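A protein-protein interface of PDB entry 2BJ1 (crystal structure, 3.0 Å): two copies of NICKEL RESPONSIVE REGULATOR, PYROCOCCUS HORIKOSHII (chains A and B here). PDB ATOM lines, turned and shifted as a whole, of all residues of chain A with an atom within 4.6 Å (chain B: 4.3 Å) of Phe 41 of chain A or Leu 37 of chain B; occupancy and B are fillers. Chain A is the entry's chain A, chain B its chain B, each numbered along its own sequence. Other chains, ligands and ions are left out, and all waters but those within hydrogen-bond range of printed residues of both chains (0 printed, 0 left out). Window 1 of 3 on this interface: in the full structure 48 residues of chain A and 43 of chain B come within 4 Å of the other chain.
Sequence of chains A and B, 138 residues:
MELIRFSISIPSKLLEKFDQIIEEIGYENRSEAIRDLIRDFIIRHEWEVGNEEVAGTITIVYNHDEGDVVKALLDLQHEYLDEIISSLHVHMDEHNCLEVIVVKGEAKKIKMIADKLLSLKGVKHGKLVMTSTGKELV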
ATOM      1  N   LEU A  37       9.908  22.788  31.549  1.00  0.00           N
ATOM      2  CA  LEU A  37      10.757  21.999  30.677  1.00  0.00           C
ATOM      3  C   LEU A  37      10.213  22.016  29.263  1.00  0.00           C
ATOM      4  O   LEU A  37      10.979  22.122  28.302  1.00  0.00           O
ATOM      5  CB  LEU A  37      10.843  20.557  31.168  1.00  0.00           C
ATOM      6  CG  LEU A  37      11.554  20.292  32.492  1.00  0.00           C
ATOM      7  CD1 LEU A  37      11.729  18.785  32.696  1.00  0.00           C
ATOM      8  CD2 LEU A  37      12.897  20.987  32.486  1.00  0.00           C
ATOM      9  N   ILE A  38       8.890  21.921  29.142  1.00  0.00           N
ATOM     10  CA  ILE A  38       8.232  21.920  27.837  1.00  0.00           C
ATOM     11  C   ILE A  38       8.319  23.294  27.175  1.00  0.00           C
ATOM     12  O   ILE A  38       8.656  23.398  25.980  1.00  0.00           O
ATOM     13  CB  ILE A  38       6.756  21.497  27.967  1.00  0.00           C
ATOM     14  CG1 ILE A  38       6.691  20.083  28.528  1.00  0.00           C
ATOM     15  CG2 ILE A  38       6.071  21.542  26.609  1.00  0.00           C
ATOM     16  CD1 ILE A  38       5.317  19.638  28.906  1.00  0.00           C
ATOM     17  N   ARG A  39       8.014  24.343  27.941  1.00  0.00           N
ATOM     18  CA  ARG A  39       8.097  25.687  27.396  1.00  0.00           C
ATOM     19  C   ARG A  39       9.510  25.920  26.894  1.00  0.00           C
ATOM     20  O   ARG A  39       9.711  26.511  25.838  1.00  0.00           O
ATOM     21  CB  ARG A  39       7.749  26.730  28.453  1.00  0.00           C
ATOM     22  CG  ARG A  39       6.273  26.870  28.697  1.00  0.00           C
ATOM     23  CD  ARG A  39       5.917  28.223  29.297  1.00  0.00           C
ATOM     24  NE  ARG A  39       4.845  28.054  30.272  1.00  0.00           N
ATOM     25  CZ  ARG A  39       5.017  27.456  31.448  1.00  0.00           C
ATOM     26  NH1 ARG A  39       6.222  26.996  31.775  1.00  0.00           N
ATOM     27  NH2 ARG A  39       3.990  27.291  32.284  1.00  0.00           N
ATOM     28  N   ASP A  40      10.483  25.438  27.660  1.00  0.00           N
ATOM     29  CA  ASP A  40      11.894  25.575  27.308  1.00  0.00           C
ATOM     30  C   ASP A  40      12.253  24.733  26.077  1.00  0.00           C
ATOM     31  O   ASP A  40      12.977  25.194  25.196  1.00  0.00           O
ATOM     32  CB  ASP A  40      12.778  25.171  28.495  1.00  0.00           C
ATOM     33  CG  ASP A  40      14.255  25.439  28.241  1.00  0.00           C
ATOM     34  OD1 ASP A  40      14.596  26.597  27.908  1.00  0.00           O
ATOM     35  OD2 ASP A  40      15.075  24.499  28.375  1.00  0.00           O
ATOM     36  N   PHE A  41      11.757  23.501  26.020  1.00  0.00           N
ATOM     37  CA  PHE A  41      12.032  22.644  24.873  1.00  0.00           C
ATOM     38  C   PHE A  41      11.534  23.333  23.609  1.00  0.00           C
ATOM     39  O   PHE A  41      12.194  23.286  22.569  1.00  0.00           O
ATOM     40  CB  PHE A  41      11.323  21.292  25.009  1.00  0.00           C
ATOM     41  CG  PHE A  41      11.436  20.420  23.780  1.00  0.00           C
ATOM     42  CD1 PHE A  41      12.588  19.693  23.522  1.00  0.00           C
ATOM     43  CD2 PHE A  41      10.397  20.366  22.856  1.00  0.00           C
ATOM     44  CE1 PHE A  41      12.698  18.931  22.364  1.00  0.00           C
ATOM     45  CE2 PHE A  41      10.509  19.604  21.696  1.00  0.00           C
ATOM     46  CZ  PHE A  41      11.653  18.893  21.451  1.00  0.00           C
ATOM     47  N   ILE A  42      10.366  23.967  23.698  1.00  0.00           N
ATOM     48  CA  ILE A  42       9.797  24.651  22.544  1.00  0.00           C
ATOM     49  C   ILE A  42      10.710  25.792  22.095  1.00  0.00           C
ATOM     50  O   ILE A  42      11.008  25.945  20.900  1.00  0.00           O
ATOM     51  CB  ILE A  42       8.406  25.195  22.865  1.00  0.00           C
ATOM     52  CG1 ILE A  42       7.556  24.089  23.488  1.00  0.00           C
ATOM     53  CG2 ILE A  42       7.742  25.690  21.596  1.00  0.00           C
ATOM     54  CD1 ILE A  42       6.072  24.412  23.591  1.00  0.00           C
ATOM     55  N   ILE A  43      11.153  26.583  23.066  1.00  0.00           N
ATOM     56  CA  ILE A  43      12.060  27.691  22.805  1.00  0.00           C
ATOM     57  C   ILE A  43      13.255  27.173  22.019  1.00  0.00           C
ATOM     58  O   ILE A  43      13.622  27.731  20.989  1.00  0.00           O
ATOM     59  CB  ILE A  43      12.584  28.296  24.127  1.00  0.00           C
ATOM     60  CG1 ILE A  43      11.565  29.275  24.700  1.00  0.00           C
ATOM     61  CG2 ILE A  43      13.930  28.968  23.909  1.00  0.00           C
ATOM     62  CD1 ILE A  43      11.970  29.834  26.053  1.00  0.00           C
ATOM     63  N   ARG A  44      13.850  26.093  22.513  1.00  0.00           N
ATOM     64  CA  ARG A  44      15.024  25.508  21.886  1.00  0.00           C
ATOM     65  C   ARG A  44      14.825  24.849  20.532  1.00  0.00           C
ATOM     66  O   ARG A  44      15.781  24.764  19.761  1.00  0.00           O
ATOM     67  CB  ARG A  44      15.699  24.503  22.832  1.00  0.00           C
ATOM     68  CG  ARG A  44      16.456  25.142  23.989  1.00  0.00           C
ATOM     69  CD  ARG A  44      17.308  24.141  24.784  1.00  0.00           C
ATOM     70  NE  ARG A  44      16.543  23.308  25.717  1.00  0.00           N
ATOM     71  CZ  ARG A  44      15.995  22.129  25.419  1.00  0.00           C
ATOM     72  NH1 ARG A  44      16.120  21.614  24.200  1.00  0.00           N
ATOM     73  NH2 ARG A  44      15.317  21.461  26.346  1.00  0.00           N
ATOM     74  N   HIS A  45      13.613  24.402  20.206  1.00  0.00           N
ATOM     75  CA  HIS A  45      13.436  23.725  18.923  1.00  0.00           C
ATOM     76  C   HIS A  45      12.475  24.307  17.891  1.00  0.00           C
ATOM     77  O   HIS A  45      12.470  23.857  16.748  1.00  0.00           O
ATOM     78  CB  HIS A  45      13.080  22.257  19.169  1.00  0.00           C
ATOM     79  CG  HIS A  45      14.120  21.502  19.935  1.00  0.00           C
ATOM     80  ND1 HIS A  45      15.215  20.922  19.337  1.00  0.00           N
ATOM     81  CD2 HIS A  45      14.246  21.259  21.262  1.00  0.00           C
ATOM     82  CE1 HIS A  45      15.970  20.353  20.260  1.00  0.00           C
ATOM     83  NE2 HIS A  45      15.403  20.544  21.438  1.00  0.00           N
ATOM     84  N   PHE B  18       4.239  21.660  21.407  1.00  0.00           N
ATOM     85  CA  PHE B  18       5.139  20.579  21.777  1.00  0.00           C
ATOM     86  C   PHE B  18       4.962  19.466  20.763  1.00  0.00           C
ATOM     87  O   PHE B  18       5.899  19.110  20.056  1.00  0.00           O
ATOM     88  CB  PHE B  18       4.788  20.076  23.175  1.00  0.00           C
ATOM     89  CG  PHE B  18       5.771  19.094  23.734  1.00  0.00           C
ATOM     90  CD1 PHE B  18       7.143  19.342  23.662  1.00  0.00           C
ATOM     91  CD2 PHE B  18       5.324  17.937  24.369  1.00  0.00           C
ATOM     92  CE1 PHE B  18       8.057  18.452  24.216  1.00  0.00           C
ATOM     93  CE2 PHE B  18       6.227  17.037  24.928  1.00  0.00           C
ATOM     94  CZ  PHE B  18       7.597  17.295  24.852  1.00  0.00           C
ATOM     95  N   ILE B  21       6.590  20.150  17.335  1.00  0.00           N
ATOM     96  CA  ILE B  21       8.047  20.050  17.346  1.00  0.00           C
ATOM     97  C   ILE B  21       8.464  18.584  17.526  1.00  0.00           C
ATOM     98  O   ILE B  21       9.231  18.051  16.729  1.00  0.00           O
ATOM     99  CB  ILE B  21       8.639  20.897  18.504  1.00  0.00           C
ATOM    100  CG1 ILE B  21       8.485  22.378  18.198  1.00  0.00           C
ATOM    101  CG2 ILE B  21      10.100  20.572  18.721  1.00  0.00           C
ATOM    102  CD1 ILE B  21       9.215  23.263  19.184  1.00  0.00           C
ATOM    103  N   ILE B  25      10.752  16.063  15.178  1.00  0.00           N
ATOM    104  CA  ILE B  25      11.998  15.389  15.564  1.00  0.00           C
ATOM    105  C   ILE B  25      12.053  13.895  15.247  1.00  0.00           C
ATOM    106  O   ILE B  25      13.128  13.331  15.045  1.00  0.00           O
ATOM    107  CB  ILE B  25      12.275  15.569  17.068  1.00  0.00           C
ATOM    108  CG1 ILE B  25      12.559  17.037  17.368  1.00  0.00           C
ATOM    109  CG2 ILE B  25      13.448  14.719  17.488  1.00  0.00           C
ATOM    110  CD1 ILE B  25      12.820  17.305  18.830  1.00  0.00           C
ATOM    111  N   ALA B  33       9.469  11.823  24.671  1.00  0.00           N
ATOM    112  CA  ALA B  33      10.136  13.118  24.635  1.00  0.00           C
ATOM    113  C   ALA B  33      10.198  13.778  26.020  1.00  0.00           C
ATOM    114  O   ALA B  33      11.237  14.313  26.417  1.00  0.00           O
ATOM    115  CB  ALA B  33       9.425  14.017  23.649  1.00  0.00           C
ATOM    116  N   ILE B  34       9.097  13.731  26.760  1.00  0.00           N
ATOM    117  CA  ILE B  34       9.073  14.331  28.081  1.00  0.00           C
ATOM    118  C   ILE B  34      10.133  13.716  28.981  1.00  0.00           C
ATOM    119  O   ILE B  34      10.732  14.406  29.805  1.00  0.00           O
ATOM    120  CB  ILE B  34       7.707  14.166  28.730  1.00  0.00           C
ATOM    121  CG1 ILE B  34       6.640  14.717  27.780  1.00  0.00           C
ATOM    122  CG2 ILE B  34       7.680  14.884  30.081  1.00  0.00           C
ATOM    123  CD1 ILE B  34       5.236  14.624  28.310  1.00  0.00           C
ATOM    124  N   ARG B  35      10.368  12.416  28.819  1.00  0.00           N
ATOM    125  CA  ARG B  35      11.376  11.735  29.622  1.00  0.00           C
ATOM    126  C   ARG B  35      12.737  12.264  29.243  1.00  0.00           C
ATOM    127  O   ARG B  35      13.598  12.450  30.098  1.00  0.00           O
ATOM    128  CB  ARG B  35      11.325  10.222  29.411  1.00  0.00           C
ATOM    129  CG  ARG B  35      10.025   9.623  29.879  1.00  0.00           C
ATOM    130  CD  ARG B  35      10.128   8.156  30.176  1.00  0.00           C
ATOM    131  NE  ARG B  35       9.018   7.436  29.569  1.00  0.00           N
ATOM    132  CZ  ARG B  35       9.026   6.975  28.321  1.00  0.00           C
ATOM    133  NH1 ARG B  35      10.099   7.154  27.546  1.00  0.00           N
ATOM    134  NH2 ARG B  35       7.960   6.335  27.847  1.00  0.00           N
ATOM    135  N   ASP B  36      12.937  12.499  27.952  1.00  0.00           N
ATOM    136  CA  ASP B  36      14.206  13.040  27.506  1.00  0.00           C
ATOM    137  C   ASP B  36      14.365  14.308  28.297  1.00  0.00           C
ATOM    138  O   ASP B  36      15.317  14.446  29.063  1.00  0.00           O
ATOM    139  CB  ASP B  36      14.180  13.345  26.009  1.00  0.00           C
ATOM    140  CG  ASP B  36      14.460  12.112  25.159  1.00  0.00           C
ATOM    141  OD1 ASP B  36      14.490  12.234  23.915  1.00  0.00           O
ATOM    142  OD2 ASP B  36      14.656  11.018  25.738  1.00  0.00           O
ATOM    143  N   LEU B  37      13.399  15.213  28.139  1.00  0.00           N
ATOM    144  CA  LEU B  37      13.407  16.494  28.844  1.00  0.00           C
ATOM    145  C   LEU B  37      13.799  16.303  30.304  1.00  0.00           C
ATOM    146  O   LEU B  37      14.689  16.980  30.814  1.00  0.00           O
ATOM    147  CB  LEU B  37      12.021  17.141  28.789  1.00  0.00           C
ATOM    148  CG  LEU B  37      11.449  17.534  27.433  1.00  0.00           C
ATOM    149  CD1 LEU B  37      10.016  18.020  27.565  1.00  0.00           C
ATOM    150  CD2 LEU B  37      12.324  18.612  26.850  1.00  0.00           C
ATOM    151  N   ILE B  38      13.121  15.364  30.959  1.00  0.00           N
ATOM    152  CA  ILE B  38      13.347  15.080  32.369  1.00  0.00           C
ATOM    153  C   ILE B  38      14.760  14.587  32.596  1.00  0.00           C
ATOM    154  O   ILE B  38      15.465  15.098  33.464  1.00  0.00           O
ATOM    155  CB  ILE B  38      12.326  14.027  32.894  1.00  0.00           C
ATOM    156  CG1 ILE B  38      10.900  14.590  32.785  1.00  0.00           C
ATOM    157  CG2 ILE B  38      12.639  13.653  34.341  1.00  0.00           C
ATOM    158  CD1 ILE B  38       9.780  13.540  32.807  1.00  0.00           C
ATOM    159  N   ARG B  39      15.167  13.599  31.801  1.00  0.00           N
ATOM    160  CA  ARG B  39      16.500  13.018  31.889  1.00  0.00           C
ATOM    161  C   ARG B  39      17.587  14.070  31.698  1.00  0.00           C
ATOM    162  O   ARG B  39      18.570  14.093  32.438  1.00  0.00           O
ATOM    163  CB  ARG B  39      16.668  11.928  30.835  1.00  0.00           C
ATOM    164  CG  ARG B  39      16.495  10.510  31.350  1.00  0.00           C
ATOM    165  CD  ARG B  39      17.120   9.501  30.386  1.00  0.00           C
ATOM    166  NE  ARG B  39      16.315   9.321  29.185  1.00  0.00           N
ATOM    167  CZ  ARG B  39      15.327   8.440  29.082  1.00  0.00           C
ATOM    168  NH1 ARG B  39      15.030   7.648  30.111  1.00  0.00           N
ATOM    169  NH2 ARG B  39      14.627   8.363  27.954  1.00  0.00           N
ATOM    170  N   ASP B  40      17.413  14.934  30.699  1.00  0.00           N
ATOM    171  CA  ASP B  40      18.384  15.987  30.422  1.00  0.00           C
ATOM    172  C   ASP B  40      18.436  16.950  31.597  1.00  0.00           C
ATOM    173  O   ASP B  40      19.514  17.294  32.096  1.00  0.00           O
ATOM    174  CB  ASP B  40      18.005  16.743  29.147  1.00  0.00           C
ATOM    175  CG  ASP B  40      18.396  15.994  27.878  1.00  0.00           C
ATOM    176  OD1 ASP B  40      17.898  14.866  27.653  1.00  0.00           O
ATOM    177  OD2 ASP B  40      19.206  16.541  27.098  1.00  0.00           O
ATOM    178  N   PHE B  41      17.256  17.376  32.040  1.00  0.00           N
ATOM    179  CA  PHE B  41      17.126  18.294  33.166  1.00  0.00           C
ATOM    180  C   PHE B  41      18.012  17.864  34.331  1.00  0.00           C
ATOM    181  O   PHE B  41      18.909  18.603  34.737  1.00  0.00           O
ATOM    182  CB  PHE B  41      15.666  18.348  33.617  1.00  0.00           C
ATOM    183  CG  PHE B  41      15.429  19.231  34.806  1.00  0.00           C
ATOM    184  CD1 PHE B  41      15.010  18.683  36.019  1.00  0.00           C
ATOM    185  CD2 PHE B  41      15.621  20.610  34.714  1.00  0.00           C
ATOM    186  CE1 PHE B  41      14.787  19.487  37.120  1.00  0.00           C
ATOM    187  CE2 PHE B  41      15.401  21.431  35.809  1.00  0.00           C
ATOM    188  CZ  PHE B  41      14.982  20.869  37.017  1.00  0.00           C
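Leu 37 of chain A touches Leu 37 of chain B. CD2 of Leu 37 of chain A touches CD2 of Phe 41 of chain B (3.5 Å). Ile 38 of chain A touches Phe 18 of chain B. Phe 18 of chain B touches Phe 41 of chain A (CE1 to CD2, 3.3 Å). Phe 41 of chain A touches Ile 21 of chain B (CE2 to CG2, 3.2 Å). Ile 25 of chain B touches Phe 41 of chain A (CD1 to CZ, 3.3 Å). Leu 37 of chain B touches Phe 41 of chain A (CD2 to CB, 3.4 Å). Ile 42 of chain A touches Phe 18 of chain B (CD1 to N, 3.96 Å). O of Ile 42 of chain A touches CD1 of Ile 21 of chain B, 3.7 Å away. Ile 21 of chain B touches His 45 of chain A.
Leu 37 of chain B touches its own counterpart, Leu 37 of chain A. Leu 37 of chain A touches Phe 41 of chain B, and with the chains exchanged Phe 41 of chain A touches Leu 37 of chain B. Of the 10 pairs that touch across the chains among the printed residues, 3 have their exchanged pair printed and touching as well.
The guanidinium group of Arg 44 of chain A is in hydrogen-bond range of a ring nitrogen (NE2) of His 45 of chain A (3.0 Å).
Printed residues of chain B that touch a printed residue of chain A: Phe 18, Ile 21, Ile 25, Leu 37 and Phe 41. Among the printed residues, 10 pairs touch across the chains. Among the printed residues, no Asp or Glu carboxylate lies within 4 Å of a Lys or Arg side-chain nitrogen of the other chain.
Leu 37 of chain B touches two residues of chain A. Of the printed residues of chain B, Ile 42 of chain A touches Phe 18 (3.96 Å) and Ile 21 (3.7 Å). Printed residues of chain B within 4 Å of His 45 of chain A: Ile 21 (3.5 Å). Of the printed residues of chain B, Leu 37 of chain A touches Leu 37 (3.9 Å) and Phe 41 (3.5 Å). Printed residues of chain A within 4 Å of Phe 18 of chain B: Ile 38 (3.8 Å), Phe 41 (3.3 Å) and Ile 42 (3.96 Å). Of the printed residues of chain A, Ile 25 of chain B touches Phe 41 (3.3 Å). Arg 44 of chain A touches none of the printed residues of chain B. The nearest printed residue of chain B that does not touch Phe 41 of chain A is Ala 33 of chain B (5.8 Å).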
